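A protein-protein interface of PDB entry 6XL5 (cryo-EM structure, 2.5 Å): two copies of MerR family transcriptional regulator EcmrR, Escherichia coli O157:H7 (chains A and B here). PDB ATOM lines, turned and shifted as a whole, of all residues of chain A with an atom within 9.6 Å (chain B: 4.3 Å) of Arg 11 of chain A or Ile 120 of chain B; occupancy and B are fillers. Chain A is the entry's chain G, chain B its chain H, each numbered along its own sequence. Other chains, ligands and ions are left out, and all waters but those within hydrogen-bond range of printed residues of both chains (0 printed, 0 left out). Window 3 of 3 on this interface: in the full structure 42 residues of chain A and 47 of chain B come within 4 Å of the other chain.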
ATOM      1  N   ILE A   3      18.476  -8.401   4.371  1.00  0.00           N
ATOM      2  CA  ILE A   3      17.534  -7.899   3.385  1.00  0.00           C
ATOM      3  C   ILE A   3      16.129  -8.428   3.643  1.00  0.00           C
ATOM      4  O   ILE A   3      15.151  -7.741   3.346  1.00  0.00           O
ATOM      5  CB  ILE A   3      18.048  -8.213   1.967  1.00  0.00           C
ATOM      6  CG1 ILE A   3      17.111  -7.651   0.909  1.00  0.00           C
ATOM      7  CG2 ILE A   3      18.216  -9.684   1.773  1.00  0.00           C
ATOM      8  CD1 ILE A   3      17.716  -7.608  -0.435  1.00  0.00           C
ATOM      9  N   GLY A   4      15.981  -9.640   4.172  1.00  0.00           N
ATOM     10  CA  GLY A   4      14.642 -10.118   4.481  1.00  0.00           C
ATOM     11  C   GLY A   4      14.004  -9.337   5.612  1.00  0.00           C
ATOM     12  O   GLY A   4      12.841  -8.924   5.523  1.00  0.00           O
ATOM     13  N   LEU A   5      14.787  -9.024   6.641  1.00  0.00           N
ATOM     14  CA  LEU A   5      14.258  -8.215   7.728  1.00  0.00           C
ATOM     15  C   LEU A   5      14.007  -6.792   7.274  1.00  0.00           C
ATOM     16  O   LEU A   5      13.021  -6.173   7.684  1.00  0.00           O
ATOM     17  CB  LEU A   5      15.227  -8.211   8.904  1.00  0.00           C
ATOM     18  CG  LEU A   5      14.548  -7.829  10.208  1.00  0.00           C
ATOM     19  CD1 LEU A   5      13.586  -8.912  10.557  1.00  0.00           C
ATOM     20  CD2 LEU A   5      15.568  -7.632  11.305  1.00  0.00           C
ATOM     21  N   PHE A   6      14.867  -6.265   6.409  1.00  0.00           N
ATOM     22  CA  PHE A   6      14.680  -4.895   5.965  1.00  0.00           C
ATOM     23  C   PHE A   6      13.488  -4.798   5.029  1.00  0.00           C
ATOM     24  O   PHE A   6      12.765  -3.799   5.038  1.00  0.00           O
ATOM     25  CB  PHE A   6      15.957  -4.387   5.310  1.00  0.00           C
ATOM     26  CG  PHE A   6      16.028  -2.906   5.213  1.00  0.00           C
ATOM     27  CD1 PHE A   6      16.110  -2.136   6.351  1.00  0.00           C
ATOM     28  CD2 PHE A   6      16.052  -2.281   3.987  1.00  0.00           C
ATOM     29  CE1 PHE A   6      16.183  -0.769   6.268  1.00  0.00           C
ATOM     30  CE2 PHE A   6      16.130  -0.914   3.900  1.00  0.00           C
ATOM     31  CZ  PHE A   6      16.195  -0.157   5.041  1.00  0.00           C
ATOM     32  N   SER A   7      13.269  -5.826   4.210  1.00  0.00           N
ATOM     33  CA  SER A   7      12.110  -5.845   3.333  1.00  0.00           C
ATOM     34  C   SER A   7      10.821  -5.961   4.128  1.00  0.00           C
ATOM     35  O   SER A   7       9.771  -5.502   3.670  1.00  0.00           O
ATOM     36  CB  SER A   7      12.218  -6.992   2.338  1.00  0.00           C
ATOM     37  OG  SER A   7      12.633  -8.175   2.972  1.00  0.00           O
ATOM     38  N   LYS A   8      10.868  -6.570   5.316  1.00  0.00           N
ATOM     39  CA  LYS A   8       9.648  -6.593   6.119  1.00  0.00           C
ATOM     40  C   LYS A   8       9.484  -5.305   6.913  1.00  0.00           C
ATOM     41  O   LYS A   8       8.355  -4.880   7.167  1.00  0.00           O
ATOM     42  CB  LYS A   8       9.603  -7.812   7.034  1.00  0.00           C
ATOM     43  CG  LYS A   8       9.726  -9.115   6.288  1.00  0.00           C
ATOM     44  CD  LYS A   8       9.100 -10.246   7.064  1.00  0.00           C
ATOM     45  CE  LYS A   8       9.650 -11.582   6.624  1.00  0.00           C
ATOM     46  NZ  LYS A   8      10.950 -11.858   7.285  1.00  0.00           N
ATOM     47  N   ILE A   9      10.592  -4.688   7.321  1.00  0.00           N
ATOM     48  CA  ILE A   9      10.532  -3.384   7.971  1.00  0.00           C
ATOM     49  C   ILE A   9       9.977  -2.351   7.003  1.00  0.00           C
ATOM     50  O   ILE A   9       9.092  -1.559   7.344  1.00  0.00           O
ATOM     51  CB  ILE A   9      11.928  -2.973   8.475  1.00  0.00           C
ATOM     52  CG1 ILE A   9      12.328  -3.773   9.708  1.00  0.00           C
ATOM     53  CG2 ILE A   9      11.983  -1.486   8.760  1.00  0.00           C
ATOM     54  CD1 ILE A   9      13.676  -3.380  10.259  1.00  0.00           C
ATOM     55  N   CYS A  10      10.475  -2.369   5.770  1.00  0.00           N
ATOM     56  CA  CYS A  10      10.078  -1.416   4.745  1.00  0.00           C
ATOM     57  C   CYS A  10       8.767  -1.784   4.065  1.00  0.00           C
ATOM     58  O   CYS A  10       8.183  -0.927   3.396  1.00  0.00           O
ATOM     59  CB  CYS A  10      11.176  -1.323   3.687  1.00  0.00           C
ATOM     60  SG  CYS A  10      12.640  -0.418   4.204  1.00  0.00           S
ATOM     61  N   ARG A  11       8.302  -3.027   4.224  1.00  0.00           N
ATOM     62  CA  ARG A  11       7.114  -3.549   3.539  1.00  0.00           C
ATOM     63  C   ARG A  11       7.264  -3.420   2.028  1.00  0.00           C
ATOM     64  O   ARG A  11       6.373  -2.933   1.331  1.00  0.00           O
ATOM     65  CB  ARG A  11       5.816  -2.885   4.008  1.00  0.00           C
ATOM     66  CG  ARG A  11       5.370  -3.225   5.414  1.00  0.00           C
ATOM     67  CD  ARG A  11       4.190  -2.352   5.797  1.00  0.00           C
ATOM     68  NE  ARG A  11       3.948  -2.310   7.233  1.00  0.00           N
ATOM     69  CZ  ARG A  11       4.441  -1.381   8.043  1.00  0.00           C
ATOM     70  NH1 ARG A  11       5.204  -0.413   7.555  1.00  0.00           N
ATOM     71  NH2 ARG A  11       4.166  -1.418   9.339  1.00  0.00           N
ATOM     72  N   VAL A  12       8.404  -3.880   1.518  1.00  0.00           N
ATOM     73  CA  VAL A  12       8.666  -3.885   0.090  1.00  0.00           C
ATOM     74  C   VAL A  12       9.307  -5.222  -0.249  1.00  0.00           C
ATOM     75  O   VAL A  12       9.750  -5.960   0.628  1.00  0.00           O
ATOM     76  CB  VAL A  12       9.571  -2.702  -0.319  1.00  0.00           C
ATOM     77  CG1 VAL A  12      11.024  -2.967   0.047  1.00  0.00           C
ATOM     78  CG2 VAL A  12       9.374  -2.326  -1.774  1.00  0.00           C
ATOM     79  N   THR A  13       9.312  -5.553  -1.534  1.00  0.00           N
ATOM     80  CA  THR A  13       9.846  -6.827  -1.983  1.00  0.00           C
ATOM     81  C   THR A  13      11.372  -6.837  -1.837  1.00  0.00           C
ATOM     82  O   THR A  13      12.013  -5.797  -1.678  1.00  0.00           O
ATOM     83  CB  THR A  13       9.397  -7.052  -3.434  1.00  0.00           C
ATOM     84  OG1 THR A  13       7.974  -6.946  -3.487  1.00  0.00           O
ATOM     85  CG2 THR A  13       9.733  -8.439  -3.957  1.00  0.00           C
ATOM     86  N   ILE A  14      11.955  -8.035  -1.882  1.00  0.00           N
ATOM     87  CA  ILE A  14      13.405  -8.163  -1.855  1.00  0.00           C
ATOM     88  C   ILE A  14      13.986  -7.714  -3.188  1.00  0.00           C
ATOM     89  O   ILE A  14      15.012  -7.027  -3.233  1.00  0.00           O
ATOM     90  CB  ILE A  14      13.801  -9.605  -1.501  1.00  0.00           C
ATOM     91  CG1 ILE A  14      13.659  -9.830  -0.001  1.00  0.00           C
ATOM     92  CG2 ILE A  14      15.214  -9.897  -1.920  1.00  0.00           C
ATOM     93  CD1 ILE A  14      14.162 -11.157   0.460  1.00  0.00           C
ATOM     94  N   THR A  16      12.941  -5.483  -5.085  1.00  0.00           N
ATOM     95  CA  THR A  16      12.996  -4.028  -5.098  1.00  0.00           C
ATOM     96  C   THR A  16      14.286  -3.524  -4.470  1.00  0.00           C
ATOM     97  O   THR A  16      14.919  -2.605  -4.994  1.00  0.00           O
ATOM     98  CB  THR A  16      11.793  -3.454  -4.363  1.00  0.00           C
ATOM     99  OG1 THR A  16      10.592  -3.937  -4.966  1.00  0.00           O
ATOM    100  CG2 THR A  16      11.799  -1.959  -4.450  1.00  0.00           C
ATOM    101  N   LEU A  17      14.692  -4.115  -3.349  1.00  0.00           N
ATOM    102  CA  LEU A  17      15.951  -3.733  -2.720  1.00  0.00           C
ATOM    103  C   LEU A  17      17.138  -4.108  -3.595  1.00  0.00           C
ATOM    104  O   LEU A  17      18.125  -3.369  -3.656  1.00  0.00           O
ATOM    105  CB  LEU A  17      16.056  -4.373  -1.340  1.00  0.00           C
ATOM    106  CG  LEU A  17      15.050  -3.819  -0.338  1.00  0.00           C
ATOM    107  CD1 LEU A  17      15.101  -4.583   0.954  1.00  0.00           C
ATOM    108  CD2 LEU A  17      15.316  -2.355  -0.094  1.00  0.00           C
ATOM    109  N   LEU A  45      16.847   2.996   6.182  1.00  0.00           N
ATOM    110  CA  LEU A  45      15.404   3.183   6.277  1.00  0.00           C
ATOM    111  C   LEU A  45      15.020   4.648   6.163  1.00  0.00           C
ATOM    112  O   LEU A  45      13.996   4.977   5.546  1.00  0.00           O
ATOM    113  CB  LEU A  45      14.895   2.608   7.598  1.00  0.00           C
ATOM    114  CG  LEU A  45      13.428   2.841   7.944  1.00  0.00           C
ATOM    115  CD1 LEU A  45      12.529   2.213   6.902  1.00  0.00           C
ATOM    116  CD2 LEU A  45      13.117   2.294   9.313  1.00  0.00           C
ATOM    117  N   PHE A  48      15.015   5.078   2.447  1.00  0.00           N
ATOM    118  CA  PHE A  48      13.916   4.399   1.769  1.00  0.00           C
ATOM    119  C   PHE A  48      12.598   5.114   1.999  1.00  0.00           C
ATOM    120  O   PHE A  48      11.719   5.080   1.135  1.00  0.00           O
ATOM    121  CB  PHE A  48      13.787   2.951   2.239  1.00  0.00           C
ATOM    122  CG  PHE A  48      12.701   2.184   1.534  1.00  0.00           C
ATOM    123  CD1 PHE A  48      12.942   1.577   0.320  1.00  0.00           C
ATOM    124  CD2 PHE A  48      11.431   2.082   2.081  1.00  0.00           C
ATOM    125  CE1 PHE A  48      11.943   0.877  -0.328  1.00  0.00           C
ATOM    126  CE2 PHE A  48      10.432   1.388   1.435  1.00  0.00           C
ATOM    127  CZ  PHE A  48      10.687   0.784   0.232  1.00  0.00           C
ATOM    128  N   HIS A  49      12.434   5.756   3.152  1.00  0.00           N
ATOM    129  CA  HIS A  49      11.239   6.564   3.362  1.00  0.00           C
ATOM    130  C   HIS A  49      11.170   7.734   2.388  1.00  0.00           C
ATOM    131  O   HIS A  49      10.096   8.050   1.867  1.00  0.00           O
ATOM    132  CB  HIS A  49      11.194   7.069   4.790  1.00  0.00           C
ATOM    133  CG  HIS A  49       9.836   7.513   5.221  1.00  0.00           C
ATOM    134  ND1 HIS A  49       9.462   8.838   5.248  1.00  0.00           N
ATOM    135  CD2 HIS A  49       8.765   6.808   5.644  1.00  0.00           C
ATOM    136  CE1 HIS A  49       8.214   8.929   5.670  1.00  0.00           C
ATOM    137  NE2 HIS A  49       7.767   7.711   5.917  1.00  0.00           N
ATOM    138  N   ALA A  52      10.246   6.301  -1.032  1.00  0.00           N
ATOM    139  CA  ALA A  52       8.821   6.001  -1.110  1.00  0.00           C
ATOM    140  C   ALA A  52       7.997   7.278  -1.202  1.00  0.00           C
ATOM    141  O   ALA A  52       7.009   7.331  -1.943  1.00  0.00           O
ATOM    142  CB  ALA A  52       8.390   5.175   0.098  1.00  0.00           C
ATOM    143  N   ARG A  55       8.287   8.415  -4.741  1.00  0.00           N
ATOM    144  CA  ARG A  55       7.706   7.487  -5.698  1.00  0.00           C
ATOM    145  C   ARG A  55       6.188   7.453  -5.628  1.00  0.00           C
ATOM    146  O   ARG A  55       5.541   7.088  -6.612  1.00  0.00           O
ATOM    147  CB  ARG A  55       8.286   6.097  -5.448  1.00  0.00           C
ATOM    148  CG  ARG A  55       8.393   5.211  -6.662  1.00  0.00           C
ATOM    149  CD  ARG A  55       8.790   3.814  -6.247  1.00  0.00           C
ATOM    150  NE  ARG A  55       7.845   3.232  -5.303  1.00  0.00           N
ATOM    151  CZ  ARG A  55       7.614   1.929  -5.187  1.00  0.00           C
ATOM    152  NH1 ARG A  55       8.263   1.072  -5.961  1.00  0.00           N
ATOM    153  NH2 ARG A  55       6.737   1.483  -4.300  1.00  0.00           N
ATOM    154  N   GLN A  56       5.607   7.818  -4.487  1.00  0.00           N
ATOM    155  CA  GLN A  56       4.158   7.926  -4.390  1.00  0.00           C
ATOM    156  C   GLN A  56       3.611   9.144  -5.119  1.00  0.00           C
ATOM    157  O   GLN A  56       2.403   9.208  -5.369  1.00  0.00           O
ATOM    158  CB  GLN A  56       3.737   7.954  -2.925  1.00  0.00           C
ATOM    159  CG  GLN A  56       3.899   6.620  -2.235  1.00  0.00           C
ATOM    160  CD  GLN A  56       3.542   6.687  -0.778  1.00  0.00           C
ATOM    161  OE1 GLN A  56       3.060   7.706  -0.298  1.00  0.00           O
ATOM    162  NE2 GLN A  56       3.791   5.603  -0.058  1.00  0.00           N
ATOM    163  N   LYS B 118       1.565   4.658   4.043  1.00  0.00           N
ATOM    164  CA  LYS B 118       1.874   3.244   4.177  1.00  0.00           C
ATOM    165  C   LYS B 118       0.697   2.533   4.818  1.00  0.00           C
ATOM    166  O   LYS B 118      -0.108   3.130   5.536  1.00  0.00           O
ATOM    167  CB  LYS B 118       3.085   2.975   5.073  1.00  0.00           C
ATOM    168  CG  LYS B 118       4.390   3.633   4.726  1.00  0.00           C
ATOM    169  CD  LYS B 118       5.271   3.567   5.958  1.00  0.00           C
ATOM    170  CE  LYS B 118       6.563   4.321   5.791  1.00  0.00           C
ATOM    171  NZ  LYS B 118       7.106   4.263   4.407  1.00  0.00           N
ATOM    172  N   GLU B 119       0.614   1.237   4.557  1.00  0.00           N
ATOM    173  CA  GLU B 119      -0.448   0.397   5.084  1.00  0.00           C
ATOM    174  C   GLU B 119       0.102  -0.412   6.253  1.00  0.00           C
ATOM    175  O   GLU B 119       1.027  -1.211   6.079  1.00  0.00           O
ATOM    176  CB  GLU B 119      -1.048  -0.503   4.009  1.00  0.00           C
ATOM    177  CG  GLU B 119      -2.338  -1.164   4.472  1.00  0.00           C
ATOM    178  CD  GLU B 119      -2.694  -2.387   3.670  1.00  0.00           C
ATOM    179  OE1 GLU B 119      -3.519  -2.257   2.742  1.00  0.00           O
ATOM    180  OE2 GLU B 119      -2.160  -3.473   3.970  1.00  0.00           O
ATOM    181  N   ILE B 120      -0.476  -0.216   7.431  1.00  0.00           N
ATOM    182  CA  ILE B 120      -0.044  -0.872   8.661  1.00  0.00           C
ATOM    183  C   ILE B 120      -1.012  -2.004   8.934  1.00  0.00           C
ATOM    184  O   ILE B 120      -2.185  -1.745   9.272  1.00  0.00           O
ATOM    185  CB  ILE B 120       0.022   0.110   9.834  1.00  0.00           C
ATOM    186  CG1 ILE B 120       0.823   1.342   9.435  1.00  0.00           C
ATOM    187  CG2 ILE B 120       0.671  -0.548  11.024  1.00  0.00           C
ATOM    188  CD1 ILE B 120       0.709   2.467  10.418  1.00  0.00           C
ATOM    189  N   PRO B 121      -0.610  -3.264   8.780  1.00  0.00           N
ATOM    190  CA  PRO B 121      -1.522  -4.385   8.983  1.00  0.00           C
ATOM    191  C   PRO B 121      -1.956  -4.508  10.432  1.00  0.00           C
ATOM    192  O   PRO B 121      -1.356  -3.949  11.353  1.00  0.00           O
ATOM    193  CB  PRO B 121      -0.698  -5.604   8.554  1.00  0.00           C
ATOM    194  CG  PRO B 121       0.467  -5.054   7.794  1.00  0.00           C
ATOM    195  CD  PRO B 121       0.735  -3.711   8.379  1.00  0.00           C
ATOM    196  N   GLU B 122      -3.045  -5.248  10.613  1.00  0.00           N
ATOM    197  CA  GLU B 122      -3.600  -5.466  11.932  1.00  0.00           C
ATOM    198  C   GLU B 122      -2.657  -6.345  12.748  1.00  0.00           C
ATOM    199  O   GLU B 122      -1.893  -7.144  12.198  1.00  0.00           O
ATOM    200  CB  GLU B 122      -4.966  -6.130  11.734  1.00  0.00           C
ATOM    201  CG  GLU B 122      -5.847  -6.295  12.911  1.00  0.00           C
ATOM    202  CD  GLU B 122      -7.235  -6.771  12.534  1.00  0.00           C
ATOM    203  OE1 GLU B 122      -7.473  -7.012  11.333  1.00  0.00           O
ATOM    204  OE2 GLU B 122      -8.088  -6.901  13.438  1.00  0.00           O
ATOM    205  N   TYR B 163       7.521  -4.006  16.242  1.00  0.00           N
ATOM    206  CA  TYR B 163       6.625  -2.846  16.176  1.00  0.00           C
ATOM    207  C   TYR B 163       6.152  -2.441  17.573  1.00  0.00           C
ATOM    208  O   TYR B 163       5.158  -2.953  18.086  1.00  0.00           O
ATOM    209  CB  TYR B 163       5.457  -3.127  15.239  1.00  0.00           C
ATOM    210  CG  TYR B 163       4.569  -1.926  15.001  1.00  0.00           C
ATOM    211  CD1 TYR B 163       5.119  -0.672  14.779  1.00  0.00           C
ATOM    212  CD2 TYR B 163       3.187  -2.054  14.940  1.00  0.00           C
ATOM    213  CE1 TYR B 163       4.325   0.426  14.548  1.00  0.00           C
ATOM    214  CE2 TYR B 163       2.384  -0.956  14.699  1.00  0.00           C
ATOM    215  CZ  TYR B 163       2.961   0.280  14.507  1.00  0.00           C
ATOM    216  OH  TYR B 163       2.173   1.381  14.269  1.00  0.00           O
ATOM    217  N   ALA B 203      -5.966  -2.996  11.016  1.00  0.00           N
ATOM    218  CA  ALA B 203      -5.143  -2.557   9.897  1.00  0.00           C
ATOM    219  C   ALA B 203      -5.650  -1.224   9.369  1.00  0.00           C
ATOM    220  O   ALA B 203      -6.849  -1.045   9.135  1.00  0.00           O
ATOM    221  CB  ALA B 203      -5.167  -3.597   8.780  1.00  0.00           C
ATOM    222  N   ILE B 204      -4.722  -0.287   9.180  1.00  0.00           N
ATOM    223  CA  ILE B 204      -5.030   1.087   8.818  1.00  0.00           C
ATOM    224  C   ILE B 204      -4.142   1.518   7.662  1.00  0.00           C
ATOM    225  O   ILE B 204      -3.087   0.938   7.404  1.00  0.00           O
ATOM    226  CB  ILE B 204      -4.851   2.054  10.005  1.00  0.00           C
ATOM    227  CG1 ILE B 204      -3.442   1.915  10.580  1.00  0.00           C
ATOM    228  CG2 ILE B 204      -5.905   1.804  11.067  1.00  0.00           C
ATOM    229  CD1 ILE B 204      -2.949   3.147  11.279  1.00  0.00           C
ATOM    230  N   ALA B 206      -2.075   4.929   6.740  1.00  0.00           N
ATOM    231  CA  ALA B 206      -1.576   6.027   7.547  1.00  0.00           C
ATOM    232  C   ALA B 206      -0.501   6.771   6.777  1.00  0.00           C
ATOM    233  O   ALA B 206       0.301   6.158   6.079  1.00  0.00           O
ATOM    234  CB  ALA B 206      -1.006   5.514   8.873  1.00  0.00           C
ATOM    235  N   ARG B 241      -0.696   7.452  15.915  1.00  0.00           N
ATOM    236  CA  ARG B 241       0.333   6.578  16.447  1.00  0.00           C
ATOM    237  C   ARG B 241       1.714   7.220  16.355  1.00  0.00           C
ATOM    238  O   ARG B 241       1.974   8.114  15.546  1.00  0.00           O
ATOM    239  CB  ARG B 241       0.359   5.253  15.691  1.00  0.00           C
ATOM    240  CG  ARG B 241      -0.956   4.527  15.654  1.00  0.00           C
ATOM    241  CD  ARG B 241      -0.755   3.136  15.116  1.00  0.00           C
ATOM    242  NE  ARG B 241      -2.013   2.539  14.696  1.00  0.00           N
ATOM    243  CZ  ARG B 241      -2.119   1.326  14.173  1.00  0.00           C
ATOM    244  NH1 ARG B 241      -1.038   0.579  14.005  1.00  0.00           N
ATOM    245  NH2 ARG B 241      -3.302   0.866  13.801  1.00  0.00           N
ATOM    246  N   GLN B 262       3.086   8.115  12.835  1.00  0.00           N
ATOM    247  CA  GLN B 262       2.106   7.525  11.933  1.00  0.00           C
ATOM    248  C   GLN B 262       0.747   8.146  12.219  1.00  0.00           C
ATOM    249  O   GLN B 262       0.238   8.041  13.333  1.00  0.00           O
ATOM    250  CB  GLN B 262       2.040   6.017  12.172  1.00  0.00           C
ATOM    251  CG  GLN B 262       3.237   5.268  11.658  1.00  0.00           C
ATOM    252  CD  GLN B 262       3.363   3.862  12.216  1.00  0.00           C
ATOM    253  OE1 GLN B 262       2.874   3.565  13.305  1.00  0.00           O
ATOM    254  NE2 GLN B 262       4.036   2.993  11.473  1.00  0.00           N
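Of the 20 printed residues of chain A, 2 touch a printed residue of chain B.
Printed residues of chain A that touch a printed residue of chain B: Arg 11 and His 49.
Hydrophobic or aromatic side chains of chain A within 4 Å of the printed part of chain B: His 49.
Of the 11 printed residues of chain B, 4 touch a printed residue of chain A.
Printed residues of chain B that touch a printed residue of chain A: Lys 118, Glu 119, Ile 120 and Pro 121.
Hydrophobic or aromatic side chains of chain B within 4 Å of the printed part of chain A: Ile 120 and Pro 121.
Among the printed residues, 4 pairs touch across the chains.
Among the printed residues, no Asp or Glu carboxylate lies within 4 Å of a Lys or Arg side-chain nitrogen of the other chain.
NH2 of Arg 11 of chain A touches CG2 of Ile 120 of chain B, 3.98 Å away.
Arg 11 of chain A touches Pro 121 of chain B.
His 49 of chain A touches Lys 118 of chain B (CD2 to NZ, 3.3 Å).
No position is printed for both chains.
O of Glu 119 of chain B lies within hydrogen-bond range of NE of Arg 11 of chain A (3.3 Å).
The backbone carbonyl oxygen (O) of Ala 206 of chain B sits at hydrogen-bond distance from the backbone NH (N) of Lys 118 of chain B (2.8 Å).
The backbone NH of Ile 120 of chain B sits at hydrogen-bond distance from the backbone carbonyl oxygen of Ile 204 of chain B, 2.9 Å away.
Ile 120 of chain B touches just one residue of chain A: Arg 11.
No residue of chain A comes within 4 Å of Ile 204 of chain B.
Of the printed residues of chain A, Lys 118 of chain B touches His 49 (3.3 Å).
Of the printed residues of chain B, His 49 of chain A touches Lys 118.
Of the printed residues of chain A, Glu 119 of chain B touches Arg 11.
The nearest residue of chain A that does not touch Ile 120 of chain B is Ile 9 of chain A (9.0 Å).
The nearest printed residue of chain B that does not touch His 49 of chain A is Ala 206 of chain B (7.6 Å).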
